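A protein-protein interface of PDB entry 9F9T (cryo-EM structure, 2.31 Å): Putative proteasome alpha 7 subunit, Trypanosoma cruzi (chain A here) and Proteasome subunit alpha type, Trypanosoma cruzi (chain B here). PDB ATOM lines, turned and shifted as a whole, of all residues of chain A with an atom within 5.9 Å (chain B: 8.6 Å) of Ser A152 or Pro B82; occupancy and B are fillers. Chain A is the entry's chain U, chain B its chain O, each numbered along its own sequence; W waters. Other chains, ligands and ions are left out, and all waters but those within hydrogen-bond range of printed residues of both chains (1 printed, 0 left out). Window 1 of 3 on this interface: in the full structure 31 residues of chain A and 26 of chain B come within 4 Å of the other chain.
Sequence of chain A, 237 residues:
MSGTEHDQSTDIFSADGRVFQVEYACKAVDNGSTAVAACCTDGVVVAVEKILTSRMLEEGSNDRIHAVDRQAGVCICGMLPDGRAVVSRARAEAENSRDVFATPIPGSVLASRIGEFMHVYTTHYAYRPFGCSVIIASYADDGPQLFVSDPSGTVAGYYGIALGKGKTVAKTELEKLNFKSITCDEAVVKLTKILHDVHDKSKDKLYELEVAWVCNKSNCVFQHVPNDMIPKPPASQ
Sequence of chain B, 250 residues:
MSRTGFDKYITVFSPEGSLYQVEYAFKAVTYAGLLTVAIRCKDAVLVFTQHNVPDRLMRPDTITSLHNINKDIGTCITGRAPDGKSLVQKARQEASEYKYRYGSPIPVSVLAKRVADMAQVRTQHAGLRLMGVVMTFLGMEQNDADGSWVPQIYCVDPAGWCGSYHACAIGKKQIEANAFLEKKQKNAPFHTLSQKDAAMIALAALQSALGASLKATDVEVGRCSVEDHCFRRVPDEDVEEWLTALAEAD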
ATOM      1  N   VAL A  22     -30.105  25.348  -1.176  1.00  0.00           N
ATOM      2  CA  VAL A  22     -30.285  24.031  -0.603  1.00  0.00           C
ATOM      3  C   VAL A  22     -31.764  23.728  -0.379  1.00  0.00           C
ATOM      4  O   VAL A  22     -32.179  22.648  -0.750  1.00  0.00           O
ATOM      5  CB  VAL A  22     -29.421  23.855   0.655  1.00  0.00           C
ATOM      6  CG1 VAL A  22     -29.717  22.554   1.374  1.00  0.00           C
ATOM      7  CG2 VAL A  22     -27.964  23.835   0.271  1.00  0.00           C
ATOM      8  N   CYS A  26     -33.861  20.455  -2.280  1.00  0.00           N
ATOM      9  CA  CYS A  26     -34.655  19.538  -1.503  1.00  0.00           C
ATOM     10  C   CYS A  26     -36.040  19.428  -2.114  1.00  0.00           C
ATOM     11  O   CYS A  26     -36.763  18.475  -1.836  1.00  0.00           O
ATOM     12  CB  CYS A  26     -34.816  20.003  -0.060  1.00  0.00           C
ATOM     13  SG  CYS A  26     -33.336  19.743   0.956  1.00  0.00           S
ATOM     14  N   GLY A 115     -22.650  12.032   3.223  1.00  0.00           N
ATOM     15  CA  GLY A 115     -22.932  13.358   3.783  1.00  0.00           C
ATOM     16  C   GLY A 115     -21.792  14.374   3.561  1.00  0.00           C
ATOM     17  O   GLY A 115     -22.030  15.504   3.179  1.00  0.00           O
ATOM     18  N   MET A 118     -21.875  15.422  -0.128  1.00  0.00           N
ATOM     19  CA  MET A 118     -22.988  16.256  -0.457  1.00  0.00           C
ATOM     20  C   MET A 118     -22.909  17.621   0.211  1.00  0.00           C
ATOM     21  O   MET A 118     -23.436  18.589  -0.348  1.00  0.00           O
ATOM     22  CB  MET A 118     -24.313  15.597  -0.088  1.00  0.00           C
ATOM     23  CG  MET A 118     -24.448  14.334  -0.969  1.00  0.00           C
ATOM     24  SD  MET A 118     -25.845  13.239  -0.686  1.00  0.00           S
ATOM     25  CE  MET A 118     -27.143  14.281  -1.360  1.00  0.00           C
ATOM     26  N   HIS A 119     -22.164  17.750   1.309  1.00  0.00           N
ATOM     27  CA  HIS A 119     -22.182  18.985   2.054  1.00  0.00           C
ATOM     28  C   HIS A 119     -21.358  19.989   1.298  1.00  0.00           C
ATOM     29  O   HIS A 119     -21.655  21.184   1.330  1.00  0.00           O
ATOM     30  CB  HIS A 119     -21.624  18.785   3.476  1.00  0.00           C
ATOM     31  CG  HIS A 119     -21.482  20.045   4.181  1.00  0.00           C
ATOM     32  ND1 HIS A 119     -20.251  20.545   4.498  1.00  0.00           N
ATOM     33  CD2 HIS A 119     -22.454  20.949   4.557  1.00  0.00           C
ATOM     34  CE1 HIS A 119     -20.446  21.770   4.983  1.00  0.00           C
ATOM     35  NE2 HIS A 119     -21.791  21.981   5.129  1.00  0.00           N
ATOM     36  N   THR A 122     -22.497  22.418  -0.996  1.00  0.00           N
ATOM     37  CA  THR A 122     -23.377  23.438  -0.435  1.00  0.00           C
ATOM     38  C   THR A 122     -22.612  24.673  -0.009  1.00  0.00           C
ATOM     39  O   THR A 122     -23.185  25.535   0.593  1.00  0.00           O
ATOM     40  CB  THR A 122     -24.249  22.987   0.739  1.00  0.00           C
ATOM     41  OG1 THR A 122     -23.489  22.754   1.898  1.00  0.00           O
ATOM     42  CG2 THR A 122     -25.033  21.758   0.395  1.00  0.00           C
ATOM     43  N   ASP A 150     -29.137  13.791   2.713  1.00  0.00           N
ATOM     44  CA  ASP A 150     -29.978  14.639   1.874  1.00  0.00           C
ATOM     45  C   ASP A 150     -29.129  15.756   1.243  1.00  0.00           C
ATOM     46  O   ASP A 150     -27.909  15.759   1.326  1.00  0.00           O
ATOM     47  CB  ASP A 150     -31.257  15.005   2.624  1.00  0.00           C
ATOM     48  CG  ASP A 150     -30.967  15.974   3.745  1.00  0.00           C
ATOM     49  OD1 ASP A 150     -31.661  15.886   4.773  1.00  0.00           O
ATOM     50  OD2 ASP A 150     -29.985  16.755   3.611  1.00  0.00           O
ATOM     51  N   PRO A 151     -29.695  16.620   0.394  1.00  0.00           N
ATOM     52  CA  PRO A 151     -28.889  17.608  -0.339  1.00  0.00           C
ATOM     53  C   PRO A 151     -28.092  18.555   0.558  1.00  0.00           C
ATOM     54  O   PRO A 151     -27.063  19.055   0.150  1.00  0.00           O
ATOM     55  CB  PRO A 151     -29.947  18.451  -1.107  1.00  0.00           C
ATOM     56  CG  PRO A 151     -31.175  17.573  -1.152  1.00  0.00           C
ATOM     57  CD  PRO A 151     -31.118  16.654   0.035  1.00  0.00           C
ATOM     58  N   SER A 152     -28.581  18.798   1.786  1.00  0.00           N
ATOM     59  CA  SER A 152     -27.847  19.580   2.768  1.00  0.00           C
ATOM     60  C   SER A 152     -26.608  18.848   3.241  1.00  0.00           C
ATOM     61  O   SER A 152     -25.645  19.504   3.629  1.00  0.00           O
ATOM     62  CB  SER A 152     -28.667  19.873   3.961  1.00  0.00           C
ATOM     63  OG  SER A 152     -28.785  18.673   4.734  1.00  0.00           O
ATOM     64  N   GLY A 153     -26.650  17.509   3.279  1.00  0.00           N
ATOM     65  CA  GLY A 153     -25.498  16.756   3.761  1.00  0.00           C
ATOM     66  C   GLY A 153     -25.716  16.227   5.182  1.00  0.00           C
ATOM     67  O   GLY A 153     -24.807  15.727   5.844  1.00  0.00           O
ATOM     68  N   THR A 154     -26.944  16.406   5.626  1.00  0.00           N
ATOM     69  CA  THR A 154     -27.370  15.860   6.884  1.00  0.00           C
ATOM     70  C   THR A 154     -27.554  14.364   6.720  1.00  0.00           C
ATOM     71  O   THR A 154     -28.142  13.916   5.756  1.00  0.00           O
ATOM     72  CB  THR A 154     -28.678  16.505   7.319  1.00  0.00           C
ATOM     73  OG1 THR A 154     -28.542  17.920   7.398  1.00  0.00           O
ATOM     74  CG2 THR A 154     -29.101  16.009   8.668  1.00  0.00           C
ATOM     75  N   ALA B  32     -31.702  26.671  14.011  1.00  0.00           N
ATOM     76  CA  ALA B  32     -31.676  25.228  14.154  1.00  0.00           C
ATOM     77  C   ALA B  32     -32.488  24.737  15.342  1.00  0.00           C
ATOM     78  O   ALA B  32     -32.763  23.547  15.399  1.00  0.00           O
ATOM     79  CB  ALA B  32     -30.251  24.749  14.226  1.00  0.00           C
ATOM     80  N   THR B  64     -26.578  12.947  17.072  1.00  0.00           N
ATOM     81  CA  THR B  64     -25.724  13.467  18.112  1.00  0.00           C
ATOM     82  C   THR B  64     -25.140  14.804  17.697  1.00  0.00           C
ATOM     83  O   THR B  64     -24.861  15.065  16.540  1.00  0.00           O
ATOM     84  CB  THR B  64     -24.679  12.430  18.539  1.00  0.00           C
ATOM     85  OG1 THR B  64     -24.198  12.863  19.811  1.00  0.00           O
ATOM     86  CG2 THR B  64     -23.549  12.268  17.546  1.00  0.00           C
ATOM     87  N   ILE B  77     -21.582  20.765  18.762  1.00  0.00           N
ATOM     88  CA  ILE B  77     -22.048  21.553  17.638  1.00  0.00           C
ATOM     89  C   ILE B  77     -23.399  22.163  17.952  1.00  0.00           C
ATOM     90  O   ILE B  77     -24.316  21.438  18.270  1.00  0.00           O
ATOM     91  CB  ILE B  77     -22.264  20.609  16.456  1.00  0.00           C
ATOM     92  CG1 ILE B  77     -20.922  20.248  15.836  1.00  0.00           C
ATOM     93  CG2 ILE B  77     -23.208  21.268  15.457  1.00  0.00           C
ATOM     94  CD1 ILE B  77     -21.005  19.070  14.863  1.00  0.00           C
ATOM     95  N   GLY B  79     -26.072  24.656  15.846  1.00  0.00           N
ATOM     96  CA  GLY B  79     -26.417  25.312  14.593  1.00  0.00           C
ATOM     97  C   GLY B  79     -26.633  24.344  13.432  1.00  0.00           C
ATOM     98  O   GLY B  79     -27.230  23.291  13.585  1.00  0.00           O
ATOM     99  N   ARG B  80     -26.232  24.791  12.248  1.00  0.00           N
ATOM    100  CA  ARG B  80     -26.525  24.040  11.049  1.00  0.00           C
ATOM    101  C   ARG B  80     -25.630  22.806  11.113  1.00  0.00           C
ATOM    102  O   ARG B  80     -24.410  22.934  11.082  1.00  0.00           O
ATOM    103  CB  ARG B  80     -26.322  24.952   9.837  1.00  0.00           C
ATOM    104  CG  ARG B  80     -26.546  24.321   8.469  1.00  0.00           C
ATOM    105  CD  ARG B  80     -26.289  25.317   7.324  1.00  0.00           C
ATOM    106  NE  ARG B  80     -26.587  24.714   6.015  1.00  0.00           N
ATOM    107  CZ  ARG B  80     -27.816  24.638   5.496  1.00  0.00           C
ATOM    108  NH1 ARG B  80     -28.822  25.247   6.093  1.00  0.00           N
ATOM    109  NH2 ARG B  80     -28.026  23.981   4.365  1.00  0.00           N
ATOM    110  N   ALA B  81     -26.272  21.631  11.268  1.00  0.00           N
ATOM    111  CA  ALA B  81     -25.610  20.411  11.691  1.00  0.00           C
ATOM    112  C   ALA B  81     -24.540  19.955  10.731  1.00  0.00           C
ATOM    113  O   ALA B  81     -23.370  19.874  11.083  1.00  0.00           O
ATOM    114  CB  ALA B  81     -26.633  19.361  11.835  1.00  0.00           C
ATOM    115  N   PRO B  82     -24.830  19.764   9.446  1.00  0.00           N
ATOM    116  CA  PRO B  82     -23.757  19.385   8.545  1.00  0.00           C
ATOM    117  C   PRO B  82     -22.627  20.391   8.427  1.00  0.00           C
ATOM    118  O   PRO B  82     -21.574  19.974   8.024  1.00  0.00           O
ATOM    119  CB  PRO B  82     -24.460  19.234   7.172  1.00  0.00           C
ATOM    120  CG  PRO B  82     -25.705  20.159   7.298  1.00  0.00           C
ATOM    121  CD  PRO B  82     -26.085  20.094   8.761  1.00  0.00           C
ATOM    122  N   ASP B  83     -22.769  21.665   8.812  1.00  0.00           N
ATOM    123  CA  ASP B  83     -21.605  22.570   8.796  1.00  0.00           C
ATOM    124  C   ASP B  83     -20.724  22.262   9.991  1.00  0.00           C
ATOM    125  O   ASP B  83     -19.508  22.159   9.847  1.00  0.00           O
ATOM    126  CB  ASP B  83     -21.963  24.068   8.780  1.00  0.00           C
ATOM    127  CG  ASP B  83     -22.613  24.592   7.492  1.00  0.00           C
ATOM    128  OD1 ASP B  83     -22.864  23.787   6.518  1.00  0.00           O
ATOM    129  OD2 ASP B  83     -22.907  25.800   7.453  1.00  0.00           O
ATOM    130  N   GLY B  84     -21.389  21.932  11.094  1.00  0.00           N
ATOM    131  CA  GLY B  84     -20.767  21.325  12.263  1.00  0.00           C
ATOM    132  C   GLY B  84     -19.838  20.167  11.898  1.00  0.00           C
ATOM    133  O   GLY B  84     -18.639  20.220  12.177  1.00  0.00           O
ATOM    134  N   LYS B  85     -20.384  19.112  11.288  1.00  0.00           N
ATOM    135  CA  LYS B  85     -19.568  17.948  10.984  1.00  0.00           C
ATOM    136  C   LYS B  85     -18.424  18.301  10.060  1.00  0.00           C
ATOM    137  O   LYS B  85     -17.363  17.687  10.203  1.00  0.00           O
ATOM    138  CB  LYS B  85     -20.276  16.789  10.279  1.00  0.00           C
ATOM    139  CG  LYS B  85     -21.678  16.512  10.771  1.00  0.00           C
ATOM    140  CD  LYS B  85     -21.816  15.485  11.899  1.00  0.00           C
ATOM    141  CE  LYS B  85     -23.220  15.516  12.502  1.00  0.00           C
ATOM    142  NZ  LYS B  85     -23.536  14.297  13.288  1.00  0.00           N
ATOM    143  N   SER B  86     -18.591  19.281   9.139  1.00  0.00           N
ATOM    144  CA  SER B  86     -17.388  19.629   8.401  1.00  0.00           C
ATOM    145  C   SER B  86     -16.266  20.123   9.332  1.00  0.00           C
ATOM    146  O   SER B  86     -15.119  19.702   9.170  1.00  0.00           O
ATOM    147  CB  SER B  86     -17.563  20.526   7.190  1.00  0.00           C
ATOM    148  OG  SER B  86     -18.180  21.731   7.555  1.00  0.00           O
ATOM    149  N   LEU B  87     -16.565  21.018  10.272  1.00  0.00           N
ATOM    150  CA  LEU B  87     -15.575  21.496  11.227  1.00  0.00           C
ATOM    151  C   LEU B  87     -15.065  20.385  12.124  1.00  0.00           C
ATOM    152  O   LEU B  87     -13.877  20.410  12.441  1.00  0.00           O
ATOM    153  CB  LEU B  87     -16.143  22.626  12.096  1.00  0.00           C
ATOM    154  CG  LEU B  87     -16.612  23.851  11.315  1.00  0.00           C
ATOM    155  CD1 LEU B  87     -17.030  25.015  12.216  1.00  0.00           C
ATOM    156  CD2 LEU B  87     -15.533  24.301  10.374  1.00  0.00           C
ATOM    157  N   VAL B  88     -15.899  19.402  12.485  1.00  0.00           N
ATOM    158  CA  VAL B  88     -15.363  18.267  13.240  1.00  0.00           C
ATOM    159  C   VAL B  88     -14.247  17.566  12.485  1.00  0.00           C
ATOM    160  O   VAL B  88     -13.182  17.311  13.054  1.00  0.00           O
ATOM    161  CB  VAL B  88     -16.454  17.275  13.602  1.00  0.00           C
ATOM    162  CG1 VAL B  88     -15.935  15.970  14.162  1.00  0.00           C
ATOM    163  CG2 VAL B  88     -17.437  17.906  14.581  1.00  0.00           C
ATOM    164  N   GLN B  89     -14.437  17.349  11.178  1.00  0.00           N
ATOM    165  CA  GLN B  89     -13.419  16.748  10.333  1.00  0.00           C
ATOM    166  C   GLN B  89     -12.191  17.628  10.226  1.00  0.00           C
ATOM    167  O   GLN B  89     -11.086  17.095  10.331  1.00  0.00           O
ATOM    168  CB  GLN B  89     -13.949  16.355   8.947  1.00  0.00           C
ATOM    169  CG  GLN B  89     -15.137  15.367   9.009  1.00  0.00           C
ATOM    170  CD  GLN B  89     -14.815  14.065   9.746  1.00  0.00           C
ATOM    171  OE1 GLN B  89     -15.403  13.699  10.764  1.00  0.00           O
ATOM    172  NE2 GLN B  89     -13.826  13.360   9.212  1.00  0.00           N
ATOM    173  N   LYS B  90     -12.308  18.946  10.100  1.00  0.00           N
ATOM    174  CA  LYS B  90     -11.063  19.740  10.014  1.00  0.00           C
ATOM    175  C   LYS B  90     -10.320  19.815  11.355  1.00  0.00           C
ATOM    176  O   LYS B  90      -9.147  19.631  11.449  1.00  0.00           O
ATOM    177  CB  LYS B  90     -11.384  21.112   9.406  1.00  0.00           C
ATOM    178  CG  LYS B  90     -11.843  21.005   7.960  1.00  0.00           C
ATOM    179  CD  LYS B  90     -11.922  22.289   7.212  1.00  0.00           C
ATOM    180  CE  LYS B  90     -13.262  22.526   6.517  1.00  0.00           C
ATOM    181  NZ  LYS B  90     -13.671  21.460   5.551  1.00  0.00           N
ATOM    182  N   ARG B 129     -19.002  29.717   1.599  1.00  0.00           N
ATOM    183  CA  ARG B 129     -19.948  30.111   2.636  1.00  0.00           C
ATOM    184  C   ARG B 129     -19.319  29.928   4.030  1.00  0.00           C
ATOM    185  O   ARG B 129     -18.440  29.074   4.228  1.00  0.00           O
ATOM    186  CB  ARG B 129     -21.205  29.256   2.528  1.00  0.00           C
ATOM    187  CG  ARG B 129     -22.358  29.744   3.341  1.00  0.00           C
ATOM    188  CD  ARG B 129     -23.483  28.918   2.817  1.00  0.00           C
ATOM    189  NE  ARG B 129     -23.324  27.459   2.868  1.00  0.00           N
ATOM    190  CZ  ARG B 129     -23.507  26.731   3.969  1.00  0.00           C
ATOM    191  NH1 ARG B 129     -23.686  27.357   5.116  1.00  0.00           N
ATOM    192  NH2 ARG B 129     -23.437  25.402   3.969  1.00  0.00           N
ATOM    193  N   MET B 131     -19.530  28.734   7.972  1.00  0.00           N
ATOM    194  CA  MET B 131     -20.176  27.625   8.672  1.00  0.00           C
ATOM    195  C   MET B 131     -21.075  28.216   9.740  1.00  0.00           C
ATOM    196  O   MET B 131     -20.654  29.042  10.507  1.00  0.00           O
ATOM    197  CB  MET B 131     -19.104  26.700   9.234  1.00  0.00           C
ATOM    198  CG  MET B 131     -18.246  25.971   8.137  1.00  0.00           C
ATOM    199  SD  MET B 131     -19.266  25.086   6.806  1.00  0.00           S
ATOM    200  CE  MET B 131     -18.979  26.128   5.378  1.00  0.00           C
ATOM    201  N   GLY B 132     -22.340  27.890   9.708  1.00  0.00           N
ATOM    202  CA  GLY B 132     -23.314  28.483  10.595  1.00  0.00           C
ATOM    203  C   GLY B 132     -23.448  27.717  11.903  1.00  0.00           C
ATOM    204  O   GLY B 132     -24.551  27.304  12.289  1.00  0.00           O
ATOM    205  N   VAL B 133     -22.311  27.675  12.614  1.00  0.00           N
ATOM    206  CA  VAL B 133     -22.232  26.969  13.883  1.00  0.00           C
ATOM    207  C   VAL B 133     -21.458  27.724  14.933  1.00  0.00           C
ATOM    208  O   VAL B 133     -20.606  28.513  14.627  1.00  0.00           O
ATOM    209  CB  VAL B 133     -21.560  25.593  13.691  1.00  0.00           C
ATOM    210  CG1 VAL B 133     -22.501  24.657  12.997  1.00  0.00           C
ATOM    211  CG2 VAL B 133     -20.300  25.685  12.887  1.00  0.00           C
ATOM    212  N   MET B 135     -18.975  26.103  17.697  1.00  0.00           N
ATOM    213  CA  MET B 135     -18.304  24.932  18.210  1.00  0.00           C
ATOM    214  C   MET B 135     -17.869  25.230  19.641  1.00  0.00           C
ATOM    215  O   MET B 135     -17.048  26.113  19.815  1.00  0.00           O
ATOM    216  CB  MET B 135     -17.096  24.564  17.370  1.00  0.00           C
ATOM    217  CG  MET B 135     -17.448  24.452  15.871  1.00  0.00           C
ATOM    218  SD  MET B 135     -18.661  23.109  15.442  1.00  0.00           S
ATOM    219  CE  MET B 135     -17.577  21.702  15.682  1.00  0.00           C
HETATM  220  O   HOH W   1     -25.425  22.462   3.829  1.00  0.00           O
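Hydrophobic or aromatic side chains of chain A that line the printed part of chain B: Val A22 and His A119. Of the 20 printed residues of chain B, 6 touch a printed residue of chain A. Hydrophobic or aromatic side chains of chain B within 4 Å of the printed part of chain A: Pro B82 and Met B131.
NE of Arg B129 is in hydrogen-bond range of O of Thr A122 (3.0 Å). The side-chain carboxylate of Asp B83 is in hydrogen-bond range of a ring nitrogen (NE2) of His A119 (2.5 Å).
NH2 of Arg B80 touches CG1 of Val A22 (3.7 Å). His A119 touches Pro B82. His A119 touches Ser B86. Arg B129 touches His A119 (NH2 to NE2, 3.97 Å). SD of Met B131 touches CE1 of His A119, 3.96 Å away. O of Ser A152 touches CG of Pro B82, 3.7 Å away. O of Gly A153 touches CB of Pro B82, 3.8 Å away. CD of Pro B82 touches OG1 of Thr A154, 3.6 Å away.
Water W1 lies within hydrogen-bond range of OG1 of Thr A122 (2.7 Å), O of Ser A152 (3.0 Å) and NH2 of Arg B80 (3.1 Å).
Ser A152 touches one residue of chain B. Pro B82 touches four residues of chain A. No residue of chain B comes within 4 Å of Pro A151. Gly A153 touches just one residue of chain B: Pro B82. Printed residues of chain A within 4 Å of Ser B86: His A119 (3.4 Å). Printed residues of chain A within 4 Å of Met B131: His A119. Of the printed residues of chain A, Asp B83 touches His A119 (2.5 Å). Of the printed residues of chain B, Thr A122 touches Arg B129 (3.0 Å). Of the printed residues of chain B, Val A22 touches Arg B80 (3.7 Å). The nearest printed residue of chain A that does not touch Pro B82 is Gly A115 (6.0 Å).
The side-chain hydroxyl of Ser A152 lies within hydrogen-bond range of the side-chain hydroxyl of Thr A154 (2.8 Å). The backbone NH (N) of Arg B80 sits at hydrogen-bond distance from the backbone carbonyl oxygen (O) of Gly B132 (3.0 Å). The side-chain sulfur (SG) of Cys A26 sits at hydrogen-bond distance from the backbone carbonyl oxygen (O) of Val A22 (3.6 Å). OG of Ser B86 sits at hydrogen-bond distance from SD of Met B131. The side-chain carboxylate (OD2) of Asp B83 lies within salt-bridge range of the guanidinium group (NH1) of Arg B129 (2.9 Å). The backbone NH (N) of Gly A153 is in hydrogen-bond range of the side-chain carboxylate (OD2) of Asp A150 (3.4 Å).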
